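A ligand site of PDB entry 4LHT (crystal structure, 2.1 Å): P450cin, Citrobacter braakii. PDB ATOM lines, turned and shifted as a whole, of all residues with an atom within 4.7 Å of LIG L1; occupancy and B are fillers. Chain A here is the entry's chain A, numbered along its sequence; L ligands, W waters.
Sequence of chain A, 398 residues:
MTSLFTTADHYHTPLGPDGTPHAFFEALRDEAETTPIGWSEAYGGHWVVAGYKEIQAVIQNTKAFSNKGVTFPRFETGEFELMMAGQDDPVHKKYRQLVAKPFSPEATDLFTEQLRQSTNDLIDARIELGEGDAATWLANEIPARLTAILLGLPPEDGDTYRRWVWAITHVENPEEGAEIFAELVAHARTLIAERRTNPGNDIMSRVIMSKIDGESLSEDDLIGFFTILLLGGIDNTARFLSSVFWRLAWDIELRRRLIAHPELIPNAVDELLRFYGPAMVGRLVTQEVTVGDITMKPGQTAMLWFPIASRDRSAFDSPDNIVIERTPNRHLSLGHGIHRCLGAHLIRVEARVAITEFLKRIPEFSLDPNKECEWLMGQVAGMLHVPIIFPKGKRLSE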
ATOM      1  N   ILE A  59      26.518  26.726  -9.947  1.00  0.00           N
ATOM      2  CA  ILE A  59      25.857  25.713 -10.747  1.00  0.00           C
ATOM      3  C   ILE A  59      25.933  24.313 -10.099  1.00  0.00           C
ATOM      4  O   ILE A  59      25.096  23.457 -10.368  1.00  0.00           O
ATOM      5  CB  ILE A  59      26.446  25.739 -12.191  1.00  0.00           C
ATOM      6  CG1 ILE A  59      25.375  25.411 -13.240  1.00  0.00           C
ATOM      7  CG2 ILE A  59      27.648  24.831 -12.274  1.00  0.00           C
ATOM      8  CD1 ILE A  59      25.893  25.461 -14.683  1.00  0.00           C
ATOM      9  N   ASN A  67      16.665  25.624 -10.656  1.00  0.00           N
ATOM     10  CA  ASN A  67      16.406  25.784 -12.097  1.00  0.00           C
ATOM     11  C   ASN A  67      15.013  26.288 -12.478  1.00  0.00           C
ATOM     12  O   ASN A  67      14.709  26.410 -13.676  1.00  0.00           O
ATOM     13  CB  ASN A  67      16.748  24.516 -12.873  1.00  0.00           C
ATOM     14  CG  ASN A  67      18.173  24.533 -13.373  1.00  0.00           C
ATOM     15  OD1 ASN A  67      19.099  24.652 -12.576  1.00  0.00           O
ATOM     16  ND2 ASN A  67      18.358  24.438 -14.691  1.00  0.00           N
ATOM     17  N   VAL A  70      15.668  29.113 -14.589  1.00  0.00           N
ATOM     18  CA  VAL A  70      16.568  28.827 -15.728  1.00  0.00           C
ATOM     19  C   VAL A  70      16.491  29.879 -16.854  1.00  0.00           C
ATOM     20  O   VAL A  70      17.525  30.278 -17.429  1.00  0.00           O
ATOM     21  CB  VAL A  70      16.347  27.415 -16.299  1.00  0.00           C
ATOM     22  CG1 VAL A  70      14.900  27.238 -16.847  1.00  0.00           C
ATOM     23  CG2 VAL A  70      17.371  27.152 -17.407  1.00  0.00           C
ATOM     24  N   MET A  84      12.870  19.091 -17.648  1.00  0.00           N
ATOM     25  CA  MET A  84      14.273  18.934 -17.284  1.00  0.00           C
ATOM     26  C   MET A  84      14.909  20.272 -16.881  1.00  0.00           C
ATOM     27  O   MET A  84      15.262  20.450 -15.722  1.00  0.00           O
ATOM     28  CB  MET A  84      15.065  18.206 -18.374  1.00  0.00           C
ATOM     29  CG  MET A  84      14.480  16.811 -18.696  1.00  0.00           C
ATOM     30  SD  MET A  84      15.216  16.064 -20.178  1.00  0.00           S
ATOM     31  CE  MET A  84      14.400  16.971 -21.492  1.00  0.00           C
ATOM     32  N   ALA A  85      15.060  21.195 -17.837  1.00  0.00           N
ATOM     33  CA  ALA A  85      15.745  22.474 -17.606  1.00  0.00           C
ATOM     34  C   ALA A  85      15.085  23.347 -16.540  1.00  0.00           C
ATOM     35  O   ALA A  85      15.752  24.133 -15.885  1.00  0.00           O
ATOM     36  CB  ALA A  85      15.868  23.280 -18.906  1.00  0.00           C
ATOM     37  N   HIS A  92      13.578  16.266 -11.684  1.00  0.00           N
ATOM     38  CA  HIS A  92      14.401  16.491 -12.882  1.00  0.00           C
ATOM     39  C   HIS A  92      15.071  15.193 -13.368  1.00  0.00           C
ATOM     40  O   HIS A  92      15.036  14.865 -14.556  1.00  0.00           O
ATOM     41  CB  HIS A  92      15.483  17.518 -12.587  1.00  0.00           C
ATOM     42  CG  HIS A  92      16.679  17.415 -13.497  1.00  0.00           C
ATOM     43  ND1 HIS A  92      17.800  16.678 -13.183  1.00  0.00           N
ATOM     44  CD2 HIS A  92      16.923  17.994 -14.705  1.00  0.00           C
ATOM     45  CE1 HIS A  92      18.682  16.796 -14.155  1.00  0.00           C
ATOM     46  NE2 HIS A  92      18.174  17.578 -15.090  1.00  0.00           N
ATOM     47  N   ARG A  96      14.623  13.324 -17.105  1.00  0.00           N
ATOM     48  CA  ARG A  96      15.775  13.220 -17.966  1.00  0.00           C
ATOM     49  C   ARG A  96      16.084  11.769 -18.289  1.00  0.00           C
ATOM     50  O   ARG A  96      16.461  11.460 -19.423  1.00  0.00           O
ATOM     51  CB  ARG A  96      17.010  13.896 -17.358  1.00  0.00           C
ATOM     52  CG  ARG A  96      18.213  13.753 -18.267  1.00  0.00           C
ATOM     53  CD  ARG A  96      19.305  14.731 -17.928  1.00  0.00           C
ATOM     54  NE  ARG A  96      20.459  14.480 -18.789  1.00  0.00           N
ATOM     55  CZ  ARG A  96      21.353  15.410 -19.091  1.00  0.00           C
ATOM     56  NH1 ARG A  96      21.188  16.646 -18.606  1.00  0.00           N
ATOM     57  NH2 ARG A  96      22.385  15.124 -19.888  1.00  0.00           N
ATOM     58  N   PHE A 103      19.440  10.400 -26.722  1.00  0.00           N
ATOM     59  CA  PHE A 103      20.483  11.441 -26.787  1.00  0.00           C
ATOM     60  C   PHE A 103      21.909  10.971 -26.557  1.00  0.00           C
ATOM     61  O   PHE A 103      22.854  11.753 -26.649  1.00  0.00           O
ATOM     62  CB  PHE A 103      20.108  12.630 -25.895  1.00  0.00           C
ATOM     63  CG  PHE A 103      19.022  13.479 -26.497  1.00  0.00           C
ATOM     64  CD1 PHE A 103      19.324  14.360 -27.534  1.00  0.00           C
ATOM     65  CD2 PHE A 103      17.718  13.335 -26.106  1.00  0.00           C
ATOM     66  CE1 PHE A 103      18.330  15.108 -28.127  1.00  0.00           C
ATOM     67  CE2 PHE A 103      16.717  14.099 -26.686  1.00  0.00           C
ATOM     68  CZ  PHE A 103      17.022  14.988 -27.707  1.00  0.00           C
ATOM     69  N   LEU A 150      13.511  14.314 -35.118  1.00  0.00           N
ATOM     70  CA  LEU A 150      13.537  13.868 -33.729  1.00  0.00           C
ATOM     71  C   LEU A 150      12.126  13.843 -33.141  1.00  0.00           C
ATOM     72  O   LEU A 150      11.765  12.931 -32.389  1.00  0.00           O
ATOM     73  CB  LEU A 150      14.404  14.794 -32.864  1.00  0.00           C
ATOM     74  CG  LEU A 150      15.932  14.936 -33.006  1.00  0.00           C
ATOM     75  CD1 LEU A 150      16.509  15.939 -31.977  1.00  0.00           C
ATOM     76  CD2 LEU A 150      16.616  13.599 -32.892  1.00  0.00           C
ATOM     77  N   ILE A 228      10.975  22.074 -24.987  1.00  0.00           N
ATOM     78  CA  ILE A 228      12.406  22.266 -24.736  1.00  0.00           C
ATOM     79  C   ILE A 228      13.248  21.665 -25.852  1.00  0.00           C
ATOM     80  O   ILE A 228      14.199  22.282 -26.283  1.00  0.00           O
ATOM     81  CB  ILE A 228      12.838  21.785 -23.317  1.00  0.00           C
ATOM     82  CG1 ILE A 228      14.189  22.379 -22.955  1.00  0.00           C
ATOM     83  CG2 ILE A 228      12.764  20.264 -23.186  1.00  0.00           C
ATOM     84  CD1 ILE A 228      14.787  21.817 -21.757  1.00  0.00           C
ATOM     85  N   LEU A 229      12.839  20.519 -26.384  1.00  0.00           N
ATOM     86  CA  LEU A 229      13.570  19.908 -27.506  1.00  0.00           C
ATOM     87  C   LEU A 229      13.544  20.806 -28.739  1.00  0.00           C
ATOM     88  O   LEU A 229      14.560  21.017 -29.363  1.00  0.00           O
ATOM     89  CB  LEU A 229      13.054  18.514 -27.815  1.00  0.00           C
ATOM     90  CG  LEU A 229      13.196  17.513 -26.662  1.00  0.00           C
ATOM     91  CD1 LEU A 229      12.657  16.135 -27.076  1.00  0.00           C
ATOM     92  CD2 LEU A 229      14.619  17.413 -26.193  1.00  0.00           C
ATOM     93  N   GLY A 232      16.092  23.707 -28.157  1.00  0.00           N
ATOM     94  CA  GLY A 232      17.495  23.325 -28.385  1.00  0.00           C
ATOM     95  C   GLY A 232      17.933  23.320 -29.836  1.00  0.00           C
ATOM     96  O   GLY A 232      19.052  23.776 -30.179  1.00  0.00           O
ATOM     97  N   GLY A 233      17.072  22.844 -30.739  1.00  0.00           N
ATOM     98  CA  GLY A 233      17.435  22.703 -32.155  1.00  0.00           C
ATOM     99  C   GLY A 233      17.286  24.000 -32.939  1.00  0.00           C
ATOM    100  O   GLY A 233      18.253  24.537 -33.483  1.00  0.00           O
ATOM    101  N   ASN A 236      19.203  27.350 -30.083  1.00  0.00           N
ATOM    102  CA  ASN A 236      20.594  27.291 -29.662  1.00  0.00           C
ATOM    103  C   ASN A 236      21.535  26.880 -30.787  1.00  0.00           C
ATOM    104  O   ASN A 236      22.519  27.557 -31.016  1.00  0.00           O
ATOM    105  CB  ASN A 236      20.788  26.367 -28.448  1.00  0.00           C
ATOM    106  CG  ASN A 236      19.893  26.751 -27.250  1.00  0.00           C
ATOM    107  OD1 ASN A 236      18.829  27.369 -27.419  1.00  0.00           O
ATOM    108  ND2 ASN A 236      20.328  26.394 -26.045  1.00  0.00           N
ATOM    109  N   THR A 237      21.215  25.793 -31.488  1.00  0.00           N
ATOM    110  CA  THR A 237      22.074  25.282 -32.543  1.00  0.00           C
ATOM    111  C   THR A 237      22.170  26.218 -33.775  1.00  0.00           C
ATOM    112  O   THR A 237      23.271  26.459 -34.318  1.00  0.00           O
ATOM    113  CB  THR A 237      21.670  23.858 -33.018  1.00  0.00           C
ATOM    114  OG1 THR A 237      21.481  22.999 -31.896  1.00  0.00           O
ATOM    115  CG2 THR A 237      22.781  23.272 -33.876  1.00  0.00           C
ATOM    116  N   PHE A 240      24.296  29.233 -32.824  1.00  0.00           N
ATOM    117  CA  PHE A 240      25.703  28.808 -32.748  1.00  0.00           C
ATOM    118  C   PHE A 240      26.333  28.643 -34.151  1.00  0.00           C
ATOM    119  O   PHE A 240      27.381  29.204 -34.464  1.00  0.00           O
ATOM    120  CB  PHE A 240      25.834  27.499 -31.960  1.00  0.00           C
ATOM    121  CG  PHE A 240      27.209  26.875 -32.043  1.00  0.00           C
ATOM    122  CD1 PHE A 240      27.373  25.623 -32.586  1.00  0.00           C
ATOM    123  CD2 PHE A 240      28.348  27.579 -31.619  1.00  0.00           C
ATOM    124  CE1 PHE A 240      28.639  25.022 -32.660  1.00  0.00           C
ATOM    125  CE2 PHE A 240      29.629  27.007 -31.712  1.00  0.00           C
ATOM    126  CZ  PHE A 240      29.782  25.714 -32.256  1.00  0.00           C
ATOM    127  N   LEU A 273      32.651  26.435 -29.680  1.00  0.00           N
ATOM    128  CA  LEU A 273      31.646  26.458 -28.592  1.00  0.00           C
ATOM    129  C   LEU A 273      32.062  27.330 -27.414  1.00  0.00           C
ATOM    130  O   LEU A 273      31.251  28.070 -26.859  1.00  0.00           O
ATOM    131  CB  LEU A 273      31.300  25.045 -28.079  1.00  0.00           C
ATOM    132  CG  LEU A 273      30.322  24.215 -28.921  1.00  0.00           C
ATOM    133  CD1 LEU A 273      30.366  22.755 -28.473  1.00  0.00           C
ATOM    134  CD2 LEU A 273      28.863  24.805 -28.882  1.00  0.00           C
ATOM    135  N   PRO A 278      26.186  30.313 -27.447  1.00  0.00           N
ATOM    136  CA  PRO A 278      25.025  31.210 -27.494  1.00  0.00           C
ATOM    137  C   PRO A 278      24.390  31.433 -26.135  1.00  0.00           C
ATOM    138  O   PRO A 278      23.750  32.459 -25.956  1.00  0.00           O
ATOM    139  CB  PRO A 278      24.004  30.449 -28.365  1.00  0.00           C
ATOM    140  CG  PRO A 278      24.775  29.367 -29.060  1.00  0.00           C
ATOM    141  CD  PRO A 278      25.928  29.039 -28.154  1.00  0.00           C
ATOM    142  N   ALA A 279      24.569  30.499 -25.219  1.00  0.00           N
ATOM    143  CA  ALA A 279      23.702  30.405 -24.042  1.00  0.00           C
ATOM    144  C   ALA A 279      24.171  31.122 -22.785  1.00  0.00           C
ATOM    145  O   ALA A 279      25.360  31.191 -22.486  1.00  0.00           O
ATOM    146  CB  ALA A 279      23.411  28.920 -23.721  1.00  0.00           C
ATOM    147  N   VAL A 281      22.177  31.061 -18.615  1.00  0.00           N
ATOM    148  CA  VAL A 281      21.066  30.509 -17.861  1.00  0.00           C
ATOM    149  C   VAL A 281      20.951  31.270 -16.531  1.00  0.00           C
ATOM    150  O   VAL A 281      21.928  31.899 -16.079  1.00  0.00           O
ATOM    151  CB  VAL A 281      21.207  28.958 -17.591  1.00  0.00           C
ATOM    152  CG1 VAL A 281      21.376  28.181 -18.897  1.00  0.00           C
ATOM    153  CG2 VAL A 281      22.379  28.651 -16.659  1.00  0.00           C
ATOM    154  N   ARG A 283      19.428  31.167 -12.333  1.00  0.00           N
ATOM    155  CA  ARG A 283      19.123  30.380 -11.159  1.00  0.00           C
ATOM    156  C   ARG A 283      18.346  31.248 -10.194  1.00  0.00           C
ATOM    157  O   ARG A 283      18.669  32.435  -9.995  1.00  0.00           O
ATOM    158  CB  ARG A 283      20.390  29.892 -10.449  1.00  0.00           C
ATOM    159  CG  ARG A 283      21.228  28.925 -11.260  1.00  0.00           C
ATOM    160  CD  ARG A 283      20.486  27.638 -11.502  1.00  0.00           C
ATOM    161  NE  ARG A 283      21.310  26.588 -12.072  1.00  0.00           N
ATOM    162  CZ  ARG A 283      21.376  26.291 -13.364  1.00  0.00           C
ATOM    163  NH1 ARG A 283      20.654  26.968 -14.245  1.00  0.00           N
ATOM    164  NH2 ARG A 283      22.105  25.260 -13.771  1.00  0.00           N
ATOM    165  N   PHE A 306      27.993  32.596 -18.940  1.00  0.00           N
ATOM    166  CA  PHE A 306      28.952  31.646 -19.484  1.00  0.00           C
ATOM    167  C   PHE A 306      29.984  32.243 -20.447  1.00  0.00           C
ATOM    168  O   PHE A 306      31.164  31.877 -20.391  1.00  0.00           O
ATOM    169  CB  PHE A 306      28.216  30.476 -20.184  1.00  0.00           C
ATOM    170  CG  PHE A 306      27.364  29.616 -19.256  1.00  0.00           C
ATOM    171  CD1 PHE A 306      26.168  29.074 -19.704  1.00  0.00           C
ATOM    172  CD2 PHE A 306      27.770  29.328 -17.962  1.00  0.00           C
ATOM    173  CE1 PHE A 306      25.373  28.273 -18.865  1.00  0.00           C
ATOM    174  CE2 PHE A 306      26.999  28.523 -17.126  1.00  0.00           C
ATOM    175  CZ  PHE A 306      25.787  27.993 -17.584  1.00  0.00           C
ATOM    176  N   LEU A 332      32.035  26.361 -20.368  1.00  0.00           N
ATOM    177  CA  LEU A 332      30.753  26.179 -19.707  1.00  0.00           C
ATOM    178  C   LEU A 332      29.612  26.409 -20.669  1.00  0.00           C
ATOM    179  O   LEU A 332      28.468  26.650 -20.245  1.00  0.00           O
ATOM    180  CB  LEU A 332      30.611  27.149 -18.530  1.00  0.00           C
ATOM    181  CG  LEU A 332      31.540  26.849 -17.334  1.00  0.00           C
ATOM    182  CD1 LEU A 332      31.640  28.012 -16.370  1.00  0.00           C
ATOM    183  CD2 LEU A 332      31.073  25.625 -16.619  1.00  0.00           C
ATOM    184  N   SER A 333      29.921  26.373 -21.965  1.00  0.00           N
ATOM    185  CA  SER A 333      28.946  26.708 -23.004  1.00  0.00           C
ATOM    186  C   SER A 333      27.757  25.718 -23.045  1.00  0.00           C
ATOM    187  O   SER A 333      26.650  26.076 -23.497  1.00  0.00           O
ATOM    188  CB  SER A 333      29.631  26.768 -24.373  1.00  0.00           C
ATOM    189  OG  SER A 333      30.407  27.956 -24.463  1.00  0.00           O
ATOM    190  N   LEU A 334      27.987  24.482 -22.575  1.00  0.00           N
ATOM    191  CA  LEU A 334      26.944  23.457 -22.539  1.00  0.00           C
ATOM    192  C   LEU A 334      26.511  23.168 -21.090  1.00  0.00           C
ATOM    193  O   LEU A 334      25.914  22.149 -20.799  1.00  0.00           O
ATOM    194  CB  LEU A 334      27.416  22.179 -23.255  1.00  0.00           C
ATOM    195  CG  LEU A 334      27.694  22.315 -24.770  1.00  0.00           C
ATOM    196  CD1 LEU A 334      28.284  21.062 -25.363  1.00  0.00           C
ATOM    197  CD2 LEU A 334      26.426  22.714 -25.539  1.00  0.00           C
ATOM    198  N   GLY A 335      26.820  24.090 -20.191  1.00  0.00           N
ATOM    199  CA  GLY A 335      26.501  23.913 -18.799  1.00  0.00           C
ATOM    200  C   GLY A 335      27.485  23.008 -18.079  1.00  0.00           C
ATOM    201  O   GLY A 335      28.600  22.815 -18.538  1.00  0.00           O
ATOM    202  N   ILE A 338      24.305  18.576 -13.068  1.00  0.00           N
ATOM    203  CA  ILE A 338      23.109  17.767 -13.339  1.00  0.00           C
ATOM    204  C   ILE A 338      22.280  18.269 -14.551  1.00  0.00           C
ATOM    205  O   ILE A 338      21.588  17.475 -15.196  1.00  0.00           O
ATOM    206  CB  ILE A 338      22.195  17.635 -12.092  1.00  0.00           C
ATOM    207  CG1 ILE A 338      21.541  18.979 -11.768  1.00  0.00           C
ATOM    208  CG2 ILE A 338      23.006  17.097 -10.876  1.00  0.00           C
ATOM    209  CD1 ILE A 338      20.432  18.894 -10.715  1.00  0.00           C
ATOM    210  N   HIS A 339      22.341  19.566 -14.851  1.00  0.00           N
ATOM    211  CA  HIS A 339      21.611  20.081 -16.024  1.00  0.00           C
ATOM    212  C   HIS A 339      22.428  20.118 -17.340  1.00  0.00           C
ATOM    213  O   HIS A 339      21.968  20.718 -18.332  1.00  0.00           O
ATOM    214  CB  HIS A 339      21.016  21.451 -15.732  1.00  0.00           C
ATOM    215  CG  HIS A 339      19.963  21.424 -14.668  1.00  0.00           C
ATOM    216  ND1 HIS A 339      18.698  20.949 -14.905  1.00  0.00           N
ATOM    217  CD2 HIS A 339      20.017  21.759 -13.361  1.00  0.00           C
ATOM    218  CE1 HIS A 339      17.997  21.029 -13.782  1.00  0.00           C
ATOM    219  NE2 HIS A 339      18.772  21.509 -12.830  1.00  0.00           N
ATOM    220  N   ARG A 340      23.603  19.475 -17.359  1.00  0.00           N
ATOM    221  CA  ARG A 340      24.487  19.544 -18.533  1.00  0.00           C
ATOM    222  C   ARG A 340      23.741  19.199 -19.810  1.00  0.00           C
ATOM    223  O   ARG A 340      22.943  18.256 -19.807  1.00  0.00           O
ATOM    224  CB  ARG A 340      25.730  18.676 -18.392  1.00  0.00           C
ATOM    225  CG  ARG A 340      26.800  19.119 -19.392  1.00  0.00           C
ATOM    226  CD  ARG A 340      28.054  18.260 -19.377  1.00  0.00           C
ATOM    227  NE  ARG A 340      29.042  18.775 -20.320  1.00  0.00           N
ATOM    228  CZ  ARG A 340      29.376  18.208 -21.486  1.00  0.00           C
ATOM    229  NH1 ARG A 340      28.788  17.078 -21.870  1.00  0.00           N
ATOM    230  NH2 ARG A 340      30.308  18.761 -22.251  1.00  0.00           N
ATOM    231  N   CYS A 341      23.963  20.001 -20.855  1.00  0.00           N
ATOM    232  CA  CYS A 341      23.223  19.904 -22.120  1.00  0.00           C
ATOM    233  C   CYS A 341      22.950  18.466 -22.601  1.00  0.00           C
ATOM    234  O   CYS A 341      23.868  17.676 -22.777  1.00  0.00           O
ATOM    235  CB  CYS A 341      23.921  20.709 -23.229  1.00  0.00           C
ATOM    236  SG  CYS A 341      23.081  20.527 -24.808  1.00  0.00           S
ATOM    237  N   LEU A 342      21.679  18.158 -22.787  1.00  0.00           N
ATOM    238  CA  LEU A 342      21.236  16.844 -23.248  1.00  0.00           C
ATOM    239  C   LEU A 342      21.670  16.623 -24.694  1.00  0.00           C
ATOM    240  O   LEU A 342      21.951  15.507 -25.120  1.00  0.00           O
ATOM    241  CB  LEU A 342      19.717  16.784 -23.219  1.00  0.00           C
ATOM    242  CG  LEU A 342      18.954  15.549 -22.745  1.00  0.00           C
ATOM    243  CD1 LEU A 342      17.578  15.504 -23.466  1.00  0.00           C
ATOM    244  CD2 LEU A 342      19.722  14.230 -22.831  1.00  0.00           C
ATOM    245  N   GLY A 343      21.692  17.706 -25.471  1.00  0.00           N
ATOM    246  CA  GLY A 343      22.039  17.561 -26.868  1.00  0.00           C
ATOM    247  C   GLY A 343      23.519  17.732 -27.169  1.00  0.00           C
ATOM    248  O   GLY A 343      23.843  17.993 -28.308  1.00  0.00           O
ATOM    249  N   LEU A 346      25.035  15.445 -29.874  1.00  0.00           N
ATOM    250  CA  LEU A 346      24.315  15.707 -31.118  1.00  0.00           C
ATOM    251  C   LEU A 346      24.747  17.000 -31.804  1.00  0.00           C
ATOM    252  O   LEU A 346      25.000  17.028 -33.022  1.00  0.00           O
ATOM    253  CB  LEU A 346      22.813  15.728 -30.870  1.00  0.00           C
ATOM    254  CG  LEU A 346      21.867  15.999 -32.033  1.00  0.00           C
ATOM    255  CD1 LEU A 346      21.952  14.917 -33.085  1.00  0.00           C
ATOM    256  CD2 LEU A 346      20.395  16.137 -31.541  1.00  0.00           C
ATOM    257  N   ILE A 347      24.866  18.079 -31.031  1.00  0.00           N
ATOM    258  CA  ILE A 347      25.372  19.319 -31.610  1.00  0.00           C
ATOM    259  C   ILE A 347      26.836  19.226 -32.125  1.00  0.00           C
ATOM    260  O   ILE A 347      27.174  19.781 -33.172  1.00  0.00           O
ATOM    261  CB  ILE A 347      25.130  20.551 -30.708  1.00  0.00           C
ATOM    262  CG1 ILE A 347      26.156  20.645 -29.591  1.00  0.00           C
ATOM    263  CG2 ILE A 347      23.707  20.555 -30.186  1.00  0.00           C
ATOM    264  CD1 ILE A 347      27.361  21.507 -29.951  1.00  0.00           C
HETATM  265  C1  LIG L   1      20.698  22.093 -21.134  1.00  0.00           C
HETATM  266  C2  LIG L   1      23.214  24.959 -24.139  1.00  0.00           C
HETATM  267  C3  LIG L   1      21.623  22.433 -28.000  1.00  0.00           C
HETATM  268  C4  LIG L   1      18.563  20.065 -25.076  1.00  0.00           C
HETATM  269  C5  LIG L   1      21.580  23.040 -21.596  1.00  0.00           C
HETATM  270  C6  LIG L   1      22.374  23.925 -20.773  1.00  0.00           C
HETATM  271  C7  LIG L   1      23.052  24.732 -21.619  1.00  0.00           C
HETATM  272  C8  LIG L   1      22.729  24.369 -22.990  1.00  0.00           C
HETATM  273  C9  LIG L   1      24.058  25.839 -21.265  1.00  0.00           C
HETATM  274  C10 LIG L   1      22.400  23.895 -19.223  1.00  0.00           C
HETATM  275  C11 LIG L   1      21.096  24.480 -18.659  1.00  0.00           C
HETATM  276  C12 LIG L   1      21.250  24.861 -17.196  1.00  0.00           C
HETATM  277  O1  LIG L   1      22.386  24.764 -16.665  1.00  0.00           O
HETATM  278  O2  LIG L   1      20.237  25.291 -16.574  1.00  0.00           O
HETATM  279  C13 LIG L   1      23.050  24.504 -25.446  1.00  0.00           C
HETATM  280  C14 LIG L   1      23.789  24.951 -26.622  1.00  0.00           C
HETATM  281  C15 LIG L   1      23.340  24.257 -27.703  1.00  0.00           C
HETATM  282  C16 LIG L   1      22.326  23.337 -27.230  1.00  0.00           C
HETATM  283  C17 LIG L   1      24.868  26.061 -26.571  1.00  0.00           C
HETATM  284  C18 LIG L   1      23.756  24.310 -29.201  1.00  0.00           C
HETATM  285  C19 LIG L   1      24.904  24.836 -29.675  1.00  0.00           C
HETATM  286  C20 LIG L   1      20.644  21.554 -27.563  1.00  0.00           C
HETATM  287  C21 LIG L   1      19.898  20.588 -28.377  1.00  0.00           C
HETATM  288  C22 LIG L   1      19.068  19.921 -27.551  1.00  0.00           C
HETATM  289  C23 LIG L   1      19.248  20.459 -26.212  1.00  0.00           C
HETATM  290  C24 LIG L   1      20.116  20.377 -29.899  1.00  0.00           C
HETATM  291  C25 LIG L   1      18.052  18.806 -27.878  1.00  0.00           C
HETATM  292  C26 LIG L   1      17.506  18.654 -29.080  1.00  0.00           C
HETATM  293  C27 LIG L   1      18.808  20.416 -23.755  1.00  0.00           C
HETATM  294  C28 LIG L   1      18.014  20.001 -22.632  1.00  0.00           C
HETATM  295  C29 LIG L   1      18.656  20.631 -21.415  1.00  0.00           C
HETATM  296  C30 LIG L   1      19.793  21.386 -21.904  1.00  0.00           C
HETATM  297  C31 LIG L   1      16.776  19.112 -22.631  1.00  0.00           C
HETATM  298  C32 LIG L   1      18.158  20.459 -19.970  1.00  0.00           C
HETATM  299  C33 LIG L   1      18.966  19.276 -19.458  1.00  0.00           C
HETATM  300  C34 LIG L   1      18.665  19.103 -17.998  1.00  0.00           C
HETATM  301  O3  LIG L   1      19.137  18.089 -17.425  1.00  0.00           O
HETATM  302  O4  LIG L   1      17.957  19.950 -17.409  1.00  0.00           O
HETATM  303  N1  LIG L   1      21.826  23.342 -22.921  1.00  0.00           N
HETATM  304  N2  LIG L   1      22.168  23.530 -25.876  1.00  0.00           N
HETATM  305  N3  LIG L   1      20.212  21.429 -26.256  1.00  0.00           N
HETATM  306  N4  LIG L   1      19.837  21.224 -23.278  1.00  0.00           N
HETATM  307 FE1  LIG L   1      21.221  22.213 -24.589  1.00  0.00          FE
HETATM  308  C1  LG2 L   2      17.434  25.514 -23.558  1.00  0.00           C
HETATM  309  C2  LG2 L   2      18.054  24.590 -22.583  1.00  0.00           C
HETATM  310  C3  LG2 L   2      18.341  25.268 -21.294  1.00  0.00           C
HETATM  311  C4  LG2 L   2      18.155  26.748 -21.351  1.00  0.00           C
HETATM  312  C5  LG2 L   2      16.811  27.048 -21.725  1.00  0.00           C
HETATM  313  C6  LG2 L   2      16.323  26.261 -22.907  1.00  0.00           C
HETATM  314  C7  LG2 L   2      17.048  24.826 -24.822  1.00  0.00           C
HETATM  315  C8  LG2 L   2      18.997  27.233 -22.514  1.00  0.00           C
HETATM  316  C9  LG2 L   2      20.460  26.968 -22.276  1.00  0.00           C
HETATM  317  C10 LG2 L   2      18.913  28.720 -22.775  1.00  0.00           C
HETATM  318  O1  LG2 L   2      18.522  26.451 -23.802  1.00  0.00           O
HETATM  319  O   HOH W   1      24.385  22.849 -16.502  1.00  0.00           O
HETATM  320  O   HOH W   2      26.529  28.349 -24.828  1.00  0.00           O
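An iron atom (FE1) of LIG L1 is bound by the side-chain sulfur of Cys 341 (2.5 Å). ND1 of His 339 sits at hydrogen-bond distance from O4 of LIG L1 (2.8 Å). An oxygen (O4) of LIG L1 lies within hydrogen-bond range of the backbone NH (N) of Ala 85. The side-chain amide nitrogen of Asn 67 sits at hydrogen-bond distance from an oxygen (O2) of LIG L1. The guanidinium group (NH1) of Arg 96 lies within salt-bridge range of an oxygen (O3) of LIG L1. ND2 of Asn 236 lies within hydrogen-bond range of O1 of LG2 L2 (2.9 Å). The guanidinium group (NH1) of Arg 283 lies within salt-bridge range of an oxygen (O2) of LIG L1, 2.9 Å away. O3 of LIG L1 sits at hydrogen-bond distance from NE2 of His 92, 2.6 Å away.
N of Cys 341 sits at hydrogen-bond distance from O of Leu 334, at 2.9 Å. NE2 of His 92 is in hydrogen-bond range of ND1 of His 339 (3.4 Å). O of Arg 340 lies within hydrogen-bond range of NH1 of Arg 96 (2.7 Å). O of Gly 232 sits at hydrogen-bond distance from OG1 of Thr 237. The side-chain sulfur of Cys 341 lies close to the backbone NH of Gly 343, 3.2 Å away. A ring nitrogen (NE2) of His 92 sits close to the backbone carbonyl oxygen of Ile 338, at 3.4 Å. The guanidinium group of Arg 283 lies close to the side-chain amide oxygen of Asn 67 (3.0 Å). O of Leu 273 lies within hydrogen-bond range of OG of Ser 333, at 2.5 Å.
Water W2 bridges O of Ser 333 (2.6 Å) and N of Ala 279 (2.9 Å).
O of Met 84 lies close to O4 of LIG L1 (3.2 Å). The side-chain amide nitrogen of Asn 236 lies close to a nitrogen (N2) of LIG L1. The backbone carbonyl oxygen (O) of Ile 338 lies close to an oxygen (O3) of LIG L1 (3.4 Å). Residues that only touch LIG L1: Val 70 (3.5 Å), Phe 103 (3.7 Å), Ile 228 (3.5 Å), Leu 229 (3.8 Å), Gly 232 (3.6 Å), Thr 237 (3.6 Å), Phe 240 (3.6 Å), Pro 278 (3.5 Å), Ala 279 (3.99 Å), Val 281 (3.7 Å), Phe 306 (3.7 Å), Ser 333 (3.4 Å), Leu 334 (3.6 Å), Gly 335 (3.4 Å), Leu 342 (3.6 Å), Gly 343 (3.8 Å) and Ile 347 (3.6 Å). Hydrophobic or aromatic side chains that line LIG L1: Val 70, Met 84, Ala 85, His 92, Phe 103, Ile 228, Phe 240, Pro 278, Ala 279, Val 281, Phe 306, Leu 334, His 339, Leu 342 and Ile 347. 27 residues have an atom within 4 Å of LIG L1: Asn 67, Val 70, Met 84, Ala 85, His 92, Arg 96, Phe 103, Ile 228, Leu 229, Gly 232, Asn 236, Thr 237, Phe 240, Pro 278, Ala 279, Val 281, Arg 283, Phe 306, Ser 333, Leu 334, Gly 335, Ile 338, His 339, Cys 341, Leu 342, Gly 343 and Ile 347. The nearest printed residue that does not touch LIG L1 is Gly 233 (4.01 Å).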
